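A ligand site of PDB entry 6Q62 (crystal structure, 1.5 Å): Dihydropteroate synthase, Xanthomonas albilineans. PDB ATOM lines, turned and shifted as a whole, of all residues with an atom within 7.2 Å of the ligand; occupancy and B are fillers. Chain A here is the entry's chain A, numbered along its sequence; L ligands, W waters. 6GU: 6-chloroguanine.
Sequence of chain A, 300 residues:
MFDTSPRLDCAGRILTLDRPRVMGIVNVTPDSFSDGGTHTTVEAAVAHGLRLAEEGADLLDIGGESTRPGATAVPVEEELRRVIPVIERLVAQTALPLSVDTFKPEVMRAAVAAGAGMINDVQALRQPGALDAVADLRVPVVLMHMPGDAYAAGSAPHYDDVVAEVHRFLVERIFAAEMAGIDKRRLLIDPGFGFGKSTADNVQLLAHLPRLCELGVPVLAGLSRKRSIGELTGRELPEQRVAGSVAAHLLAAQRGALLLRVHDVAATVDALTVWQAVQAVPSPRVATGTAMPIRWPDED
The side-chain carboxylate (OD2) of Asp 190 sits at hydrogen-bond distance from a nitrogen (N1) of the ligand (2.6 Å). The side-chain amide oxygen (OD1) of Asn 120 sits at hydrogen-bond distance from a nitrogen (N2) of the ligand, at 2.7 Å. The side-chain amino group of Lys 226 sits at hydrogen-bond distance from a nitrogen (N7) of the ligand (3.2 Å). The guanidinium group of Arg 261 lies close to a nitrogen (N7) of the ligand, at 3.2 Å.
The side-chain sulfur (SD) of Met 144 sits close to a nitrogen (N1) of the ligand, at 3.6 Å. Asp 101 touches the ligand. Val 122 touches the ligand (CG1 to N3, 3.96 Å). Val 142 touches the ligand. Phe 195 touches the ligand. CD2 of Leu 220 touches N1 of the ligand, at 3.9 Å. Gly 222 touches the ligand (O to CL6, 3.2 Å). Within 4 Å of the ligand: Asp 101, Asn 120, Val 122, Val 142, Met 144, Asp 190, Phe 195, Leu 220, Gly 222, Lys 226 and Arg 261.
The side-chain carboxylate of Asp 190 lies within hydrogen-bond range of the backbone NH of Gly 192, at 2.8 Å. ND2 of Asn 120 is in hydrogen-bond range of OD2 of Asp 61, at 3.0 Å. The backbone carbonyl oxygen of Gly 222 sits at hydrogen-bond distance from the side-chain amino group of Lys 226. O of Phe 193 is in hydrogen-bond range of NZ of Lys 226, 2.8 Å away. NE of Arg 261 is in salt-bridge range of OD2 of Asp 61 (2.9 Å). The backbone NH (N) of Met 144 lies within hydrogen-bond range of the backbone carbonyl oxygen (O) of Asp 121 (3.5 Å). N of Asp 121 is in hydrogen-bond range of O of Val 142 (3.1 Å). The backbone NH (N) of Leu 220 is in hydrogen-bond range of the backbone carbonyl oxygen (O) of Ile 189 (2.8 Å).
Water W2 bridges a nitrogen (N9) of the ligand and the side-chain carboxylate of Asp 101. Water W1 lies within hydrogen-bond range of OD1 of Asp 190, N of Phe 193 and N of Gly 222.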
ATOM      1  N   MET A  23       9.695  27.700  -1.724  1.00  0.00           N
ATOM      2  CA  MET A  23      10.733  27.684  -0.680  1.00  0.00           C
ATOM      3  C   MET A  23      11.134  29.133  -0.383  1.00  0.00           C
ATOM      4  O   MET A  23      11.785  29.752  -1.209  1.00  0.00           O
ATOM      5  CB  MET A  23      11.961  26.880  -1.140  1.00  0.00           C
ATOM      6  CG  MET A  23      13.114  26.878  -0.134  1.00  0.00           C
ATOM      7  SD  MET A  23      14.640  26.208  -0.874  1.00  0.00           S
ATOM      8  CE  MET A  23      14.688  24.576  -0.127  1.00  0.00           C
ATOM      9  N   ILE A  25      13.220  32.177   1.143  1.00  0.00           N
ATOM     10  CA  ILE A  25      14.606  32.439   1.533  1.00  0.00           C
ATOM     11  C   ILE A  25      14.701  33.196   2.841  1.00  0.00           C
ATOM     12  O   ILE A  25      14.212  34.322   2.932  1.00  0.00           O
ATOM     13  CB  ILE A  25      15.362  33.180   0.400  1.00  0.00           C
ATOM     14  CG1 ILE A  25      15.410  32.333  -0.884  1.00  0.00           C
ATOM     15  CG2 ILE A  25      16.766  33.586   0.855  1.00  0.00           C
ATOM     16  CD1 ILE A  25      15.934  33.080  -2.142  1.00  0.00           C
ATOM     17  N   ASN A  27      17.678  34.491   4.992  1.00  0.00           N
ATOM     18  CA  ASN A  27      19.110  34.680   5.188  1.00  0.00           C
ATOM     19  C   ASN A  27      19.361  35.248   6.567  1.00  0.00           C
ATOM     20  O   ASN A  27      18.738  36.230   6.972  1.00  0.00           O
ATOM     21  CB  ASN A  27      19.691  35.575   4.100  1.00  0.00           C
ATOM     22  CG  ASN A  27      19.800  34.914   2.761  1.00  0.00           C
ATOM     23  OD1 ASN A  27      20.129  33.735   2.629  1.00  0.00           O
ATOM     24  ND2 ASN A  27      19.549  35.674   1.716  1.00  0.00           N
ATOM     25  N   ASP A  61      13.954  28.164   3.828  1.00  0.00           N
ATOM     26  CA  ASP A  61      15.344  27.759   3.696  1.00  0.00           C
ATOM     27  C   ASP A  61      16.166  28.757   4.511  1.00  0.00           C
ATOM     28  O   ASP A  61      16.284  29.924   4.141  1.00  0.00           O
ATOM     29  CB  ASP A  61      15.769  27.812   2.237  1.00  0.00           C
ATOM     30  CG  ASP A  61      17.136  27.218   1.984  1.00  0.00           C
ATOM     31  OD1 ASP A  61      17.431  26.148   2.564  1.00  0.00           O
ATOM     32  OD2 ASP A  61      17.911  27.815   1.191  1.00  0.00           O
ATOM     33  N   GLU A  65      25.310  31.606   5.598  1.00  0.00           N
ATOM     34  CA  GLU A  65      26.512  31.854   4.794  1.00  0.00           C
ATOM     35  C   GLU A  65      26.158  32.176   3.346  1.00  0.00           C
ATOM     36  O   GLU A  65      25.600  31.330   2.650  1.00  0.00           O
ATOM     37  CB  GLU A  65      27.472  30.651   4.901  1.00  0.00           C
ATOM     38  CG  GLU A  65      28.780  30.818   4.145  1.00  0.00           C
ATOM     39  CD  GLU A  65      29.810  29.740   4.394  1.00  0.00           C
ATOM     40  OE1 GLU A  65      29.413  28.574   4.634  1.00  0.00           O
ATOM     41  OE2 GLU A  65      31.024  30.053   4.333  1.00  0.00           O
ATOM     42  N   ASP A 101      20.346  25.693   4.745  1.00  0.00           N
ATOM     43  CA  ASP A 101      21.200  25.913   3.571  1.00  0.00           C
ATOM     44  C   ASP A 101      22.656  25.980   4.062  1.00  0.00           C
ATOM     45  O   ASP A 101      23.125  27.014   4.560  1.00  0.00           O
ATOM     46  CB  ASP A 101      20.754  27.225   2.918  1.00  0.00           C
ATOM     47  CG  ASP A 101      21.505  27.701   1.713  1.00  0.00           C
ATOM     48  OD1 ASP A 101      22.539  27.102   1.377  1.00  0.00           O
ATOM     49  OD2 ASP A 101      21.056  28.682   1.098  1.00  0.00           O
ATOM     50  N   ASN A 120      19.835  21.777   2.324  1.00  0.00           N
ATOM     51  CA  ASN A 120      19.989  22.339   0.988  1.00  0.00           C
ATOM     52  C   ASN A 120      21.483  22.583   0.846  1.00  0.00           C
ATOM     53  O   ASN A 120      22.014  23.501   1.454  1.00  0.00           O
ATOM     54  CB  ASN A 120      19.151  23.618   0.831  1.00  0.00           C
ATOM     55  CG  ASN A 120      19.527  24.362  -0.419  1.00  0.00           C
ATOM     56  OD1 ASN A 120      20.009  23.764  -1.376  1.00  0.00           O
ATOM     57  ND2 ASN A 120      19.327  25.675  -0.427  1.00  0.00           N
ATOM     58  N   ASP A 121      22.146  21.737   0.068  1.00  0.00           N
ATOM     59  CA  ASP A 121      23.601  21.813  -0.049  1.00  0.00           C
ATOM     60  C   ASP A 121      24.127  22.277  -1.394  1.00  0.00           C
ATOM     61  O   ASP A 121      24.138  21.508  -2.349  1.00  0.00           O
ATOM     62  CB  ASP A 121      24.213  20.456   0.336  1.00  0.00           C
ATOM     63  CG  ASP A 121      25.734  20.455   0.424  1.00  0.00           C
ATOM     64  OD1 ASP A 121      26.345  21.521   0.204  1.00  0.00           O
ATOM     65  OD2 ASP A 121      26.299  19.398   0.688  1.00  0.00           O
ATOM     66  N   VAL A 122      24.661  23.504  -1.430  1.00  0.00           N
ATOM     67  CA  VAL A 122      25.244  24.097  -2.630  1.00  0.00           C
ATOM     68  C   VAL A 122      26.445  23.287  -3.150  1.00  0.00           C
ATOM     69  O   VAL A 122      26.777  23.403  -4.333  1.00  0.00           O
ATOM     70  CB  VAL A 122      25.603  25.612  -2.472  1.00  0.00           C
ATOM     71  CG1 VAL A 122      24.354  26.457  -2.246  1.00  0.00           C
ATOM     72  CG2 VAL A 122      26.640  25.846  -1.369  1.00  0.00           C
ATOM     73  N   VAL A 142      18.945  18.594  -0.985  1.00  0.00           N
ATOM     74  CA  VAL A 142      19.044  19.191  -2.305  1.00  0.00           C
ATOM     75  C   VAL A 142      20.495  19.090  -2.761  1.00  0.00           C
ATOM     76  O   VAL A 142      21.372  19.603  -2.077  1.00  0.00           O
ATOM     77  CB  VAL A 142      18.601  20.683  -2.314  1.00  0.00           C
ATOM     78  CG1 VAL A 142      18.696  21.270  -3.734  1.00  0.00           C
ATOM     79  CG2 VAL A 142      17.192  20.876  -1.743  1.00  0.00           C
ATOM     80  N   LEU A 143      20.720  18.528  -3.949  1.00  0.00           N
ATOM     81  CA  LEU A 143      22.022  18.437  -4.559  1.00  0.00           C
ATOM     82  C   LEU A 143      22.085  19.483  -5.666  1.00  0.00           C
ATOM     83  O   LEU A 143      21.433  19.350  -6.696  1.00  0.00           O
ATOM     84  CB  LEU A 143      22.250  17.025  -5.127  1.00  0.00           C
ATOM     85  CG  LEU A 143      22.015  15.827  -4.164  1.00  0.00           C
ATOM     86  CD1 LEU A 143      22.125  14.503  -4.912  1.00  0.00           C
ATOM     87  CD2 LEU A 143      23.013  15.845  -2.965  1.00  0.00           C
ATOM     88  N   MET A 144      22.858  20.526  -5.448  1.00  0.00           N
ATOM     89  CA  MET A 144      22.941  21.616  -6.407  1.00  0.00           C
ATOM     90  C   MET A 144      24.213  21.538  -7.229  1.00  0.00           C
ATOM     91  O   MET A 144      25.222  20.994  -6.760  1.00  0.00           O
ATOM     92  CB  MET A 144      22.876  22.956  -5.634  1.00  0.00           C
ATOM     93  CG  MET A 144      22.515  24.167  -6.514  1.00  0.00           C
ATOM     94  SD  MET A 144      22.947  25.744  -5.734  1.00  0.00           S
ATOM     95  CE  MET A 144      24.707  25.809  -6.094  1.00  0.00           C
ATOM     96  N   ILE A 189      17.237  17.728  -6.889  1.00  0.00           N
ATOM     97  CA  ILE A 189      18.395  18.251  -7.624  1.00  0.00           C
ATOM     98  C   ILE A 189      18.133  19.690  -8.027  1.00  0.00           C
ATOM     99  O   ILE A 189      16.980  20.123  -8.071  1.00  0.00           O
ATOM    100  CB  ILE A 189      18.812  17.372  -8.816  1.00  0.00           C
ATOM    101  CG1 ILE A 189      17.639  17.234  -9.856  1.00  0.00           C
ATOM    102  CG2 ILE A 189      19.367  16.036  -8.315  1.00  0.00           C
ATOM    103  CD1 ILE A 189      18.007  16.450 -11.137  1.00  0.00           C
ATOM    104  N   ASP A 190      19.200  20.436  -8.306  1.00  0.00           N
ATOM    105  CA  ASP A 190      19.041  21.847  -8.626  1.00  0.00           C
ATOM    106  C   ASP A 190      20.187  22.204  -9.582  1.00  0.00           C
ATOM    107  O   ASP A 190      21.352  21.947  -9.235  1.00  0.00           O
ATOM    108  CB  ASP A 190      19.155  22.615  -7.308  1.00  0.00           C
ATOM    109  CG  ASP A 190      19.035  24.116  -7.396  1.00  0.00           C
ATOM    110  OD1 ASP A 190      19.297  24.680  -8.478  1.00  0.00           O
ATOM    111  OD2 ASP A 190      18.738  24.732  -6.370  1.00  0.00           O
ATOM    112  N   PRO A 191      19.895  22.822 -10.746  1.00  0.00           N
ATOM    113  CA  PRO A 191      20.983  23.197 -11.679  1.00  0.00           C
ATOM    114  C   PRO A 191      21.880  24.306 -11.209  1.00  0.00           C
ATOM    115  O   PRO A 191      22.886  24.623 -11.873  1.00  0.00           O
ATOM    116  CB  PRO A 191      20.236  23.603 -12.947  1.00  0.00           C
ATOM    117  CG  PRO A 191      18.921  24.097 -12.453  1.00  0.00           C
ATOM    118  CD  PRO A 191      18.569  23.188 -11.293  1.00  0.00           C
ATOM    119  N   GLY A 192      21.509  24.967 -10.120  1.00  0.00           N
ATOM    120  CA  GLY A 192      22.317  26.029  -9.537  1.00  0.00           C
ATOM    121  C   GLY A 192      22.405  27.268 -10.382  1.00  0.00           C
ATOM    122  O   GLY A 192      23.508  27.678 -10.782  1.00  0.00           O
ATOM    123  N   PHE A 193      21.240  27.862 -10.707  1.00  0.00           N
ATOM    124  CA  PHE A 193      21.258  29.090 -11.509  1.00  0.00           C
ATOM    125  C   PHE A 193      22.132  30.160 -10.852  1.00  0.00           C
ATOM    126  O   PHE A 193      22.051  30.374  -9.643  1.00  0.00           O
ATOM    127  CB  PHE A 193      19.823  29.617 -11.710  1.00  0.00           C
ATOM    128  CG  PHE A 193      18.975  28.722 -12.570  1.00  0.00           C
ATOM    129  CD1 PHE A 193      19.143  28.694 -13.943  1.00  0.00           C
ATOM    130  CD2 PHE A 193      17.926  27.988 -12.022  1.00  0.00           C
ATOM    131  CE1 PHE A 193      18.338  27.878 -14.755  1.00  0.00           C
ATOM    132  CE2 PHE A 193      17.097  27.195 -12.835  1.00  0.00           C
ATOM    133  CZ  PHE A 193      17.311  27.142 -14.199  1.00  0.00           C
ATOM    134  N   GLY A 194      22.994  30.781 -11.648  1.00  0.00           N
ATOM    135  CA  GLY A 194      23.866  31.855 -11.189  1.00  0.00           C
ATOM    136  C   GLY A 194      25.196  31.428 -10.572  1.00  0.00           C
ATOM    137  O   GLY A 194      26.044  32.290 -10.335  1.00  0.00           O
ATOM    138  N   PHE A 195      25.387  30.122 -10.310  1.00  0.00           N
ATOM    139  CA  PHE A 195      26.645  29.635  -9.718  1.00  0.00           C
ATOM    140  C   PHE A 195      27.614  29.210 -10.813  1.00  0.00           C
ATOM    141  O   PHE A 195      27.480  28.113 -11.376  1.00  0.00           O
ATOM    142  CB  PHE A 195      26.369  28.477  -8.751  1.00  0.00           C
ATOM    143  CG  PHE A 195      25.703  28.930  -7.473  1.00  0.00           C
ATOM    144  CD1 PHE A 195      24.318  29.012  -7.396  1.00  0.00           C
ATOM    145  CD2 PHE A 195      26.457  29.224  -6.342  1.00  0.00           C
ATOM    146  CE1 PHE A 195      23.698  29.377  -6.197  1.00  0.00           C
ATOM    147  CE2 PHE A 195      25.830  29.595  -5.147  1.00  0.00           C
ATOM    148  CZ  PHE A 195      24.456  29.675  -5.090  1.00  0.00           C
ATOM    149  N   LEU A 220      14.565  21.618  -8.041  1.00  0.00           N
ATOM    150  CA  LEU A 220      14.441  22.922  -7.393  1.00  0.00           C
ATOM    151  C   LEU A 220      15.078  23.945  -8.335  1.00  0.00           C
ATOM    152  O   LEU A 220      16.165  23.682  -8.869  1.00  0.00           O
ATOM    153  CB  LEU A 220      15.186  22.896  -6.040  1.00  0.00           C
ATOM    154  CG  LEU A 220      15.109  24.143  -5.152  1.00  0.00           C
ATOM    155  CD1 LEU A 220      15.340  23.773  -3.704  1.00  0.00           C
ATOM    156  CD2 LEU A 220      16.045  25.250  -5.571  1.00  0.00           C
ATOM    157  N   ALA A 221      14.434  25.103  -8.519  1.00  0.00           N
ATOM    158  CA  ALA A 221      14.991  26.179  -9.358  1.00  0.00           C
ATOM    159  C   ALA A 221      15.005  27.416  -8.483  1.00  0.00           C
ATOM    160  O   ALA A 221      14.025  27.725  -7.860  1.00  0.00           O
ATOM    161  CB  ALA A 221      14.107  26.445 -10.574  1.00  0.00           C
ATOM    162  N   GLY A 222      16.129  28.108  -8.465  1.00  0.00           N
ATOM    163  CA  GLY A 222      16.283  29.341  -7.716  1.00  0.00           C
ATOM    164  C   GLY A 222      16.857  30.429  -8.608  1.00  0.00           C
ATOM    165  O   GLY A 222      18.061  30.419  -8.864  1.00  0.00           O
ATOM    166  N   LEU A 223      16.037  31.361  -9.106  1.00  0.00           N
ATOM    167  CA  LEU A 223      16.572  32.439  -9.953  1.00  0.00           C
ATOM    168  C   LEU A 223      16.282  33.777  -9.284  1.00  0.00           C
ATOM    169  O   LEU A 223      16.518  34.830  -9.881  1.00  0.00           O
ATOM    170  CB  LEU A 223      15.883  32.398 -11.349  1.00  0.00           C
ATOM    171  CG  LEU A 223      16.069  31.145 -12.200  1.00  0.00           C
ATOM    172  CD1 LEU A 223      14.783  30.352 -12.281  1.00  0.00           C
ATOM    173  CD2 LEU A 223      16.459  31.513 -13.594  1.00  0.00           C
ATOM    174  N   SER A 224      15.830  33.732  -8.049  1.00  0.00           N
ATOM    175  CA  SER A 224      15.338  34.904  -7.316  1.00  0.00           C
ATOM    176  C   SER A 224      16.303  36.081  -7.217  1.00  0.00           C
ATOM    177  O   SER A 224      17.317  36.035  -6.547  1.00  0.00           O
ATOM    178  CB  SER A 224      14.840  34.503  -5.945  1.00  0.00           C
ATOM    179  OG  SER A 224      14.127  35.588  -5.395  1.00  0.00           O
ATOM    180  N   LYS A 226      18.358  37.277  -9.070  1.00  0.00           N
ATOM    181  CA  LYS A 226      19.737  37.030  -9.467  1.00  0.00           C
ATOM    182  C   LYS A 226      20.210  37.951 -10.584  1.00  0.00           C
ATOM    183  O   LYS A 226      19.395  38.554 -11.308  1.00  0.00           O
ATOM    184  CB  LYS A 226      19.946  35.566  -9.803  1.00  0.00           C
ATOM    185  CG  LYS A 226      19.846  34.723  -8.513  1.00  0.00           C
ATOM    186  CD  LYS A 226      20.220  33.300  -8.716  1.00  0.00           C
ATOM    187  CE  LYS A 226      20.419  32.681  -7.346  1.00  0.00           C
ATOM    188  NZ  LYS A 226      20.581  31.241  -7.463  1.00  0.00           N
ATOM    189  N   ARG A 261      12.823  28.467  -5.203  1.00  0.00           N
ATOM    190  CA  ARG A 261      13.525  29.109  -4.072  1.00  0.00           C
ATOM    191  C   ARG A 261      13.472  30.608  -4.287  1.00  0.00           C
ATOM    192  O   ARG A 261      14.186  31.133  -5.160  1.00  0.00           O
ATOM    193  CB  ARG A 261      14.959  28.571  -3.954  1.00  0.00           C
ATOM    194  CG  ARG A 261      15.700  29.159  -2.728  1.00  0.00           C
ATOM    195  CD  ARG A 261      17.077  28.530  -2.541  1.00  0.00           C
ATOM    196  NE  ARG A 261      17.731  29.123  -1.361  1.00  0.00           N
ATOM    197  CZ  ARG A 261      18.398  30.271  -1.365  1.00  0.00           C
ATOM    198  NH1 ARG A 261      18.540  30.971  -2.487  1.00  0.00           N
ATOM    199  NH2 ARG A 261      18.930  30.743  -0.244  1.00  0.00           N
HETATM  200 CL6  6GU L   1      19.736  28.648  -6.798  1.00  0.00          CL
HETATM  201  N1  6GU L   1      19.592  26.824  -5.117  1.00  0.00           N
HETATM  202  C2  6GU L   1      19.889  26.333  -3.848  1.00  0.00           C
HETATM  203  N2  6GU L   1      19.575  25.053  -3.690  1.00  0.00           N
HETATM  204  N3  6GU L   1      20.479  27.032  -2.813  1.00  0.00           N
HETATM  205  C4  6GU L   1      20.806  28.332  -3.147  1.00  0.00           C
HETATM  206  C5  6GU L   1      20.565  28.897  -4.417  1.00  0.00           C
HETATM  207  C6  6GU L   1      19.965  28.074  -5.316  1.00  0.00           C
HETATM  208  N7  6GU L   1      21.030  30.213  -4.428  1.00  0.00           N
HETATM  209  C8  6GU L   1      21.550  30.395  -3.153  1.00  0.00           C
HETATM  210  N9  6GU L   1      21.430  29.295  -2.360  1.00  0.00           N
HETATM  211  O   HOH W   1      18.949  27.259  -8.962  1.00  0.00           O
HETATM  212  O   HOH W   2      23.028  29.787  -0.302  1.00  0.00           O
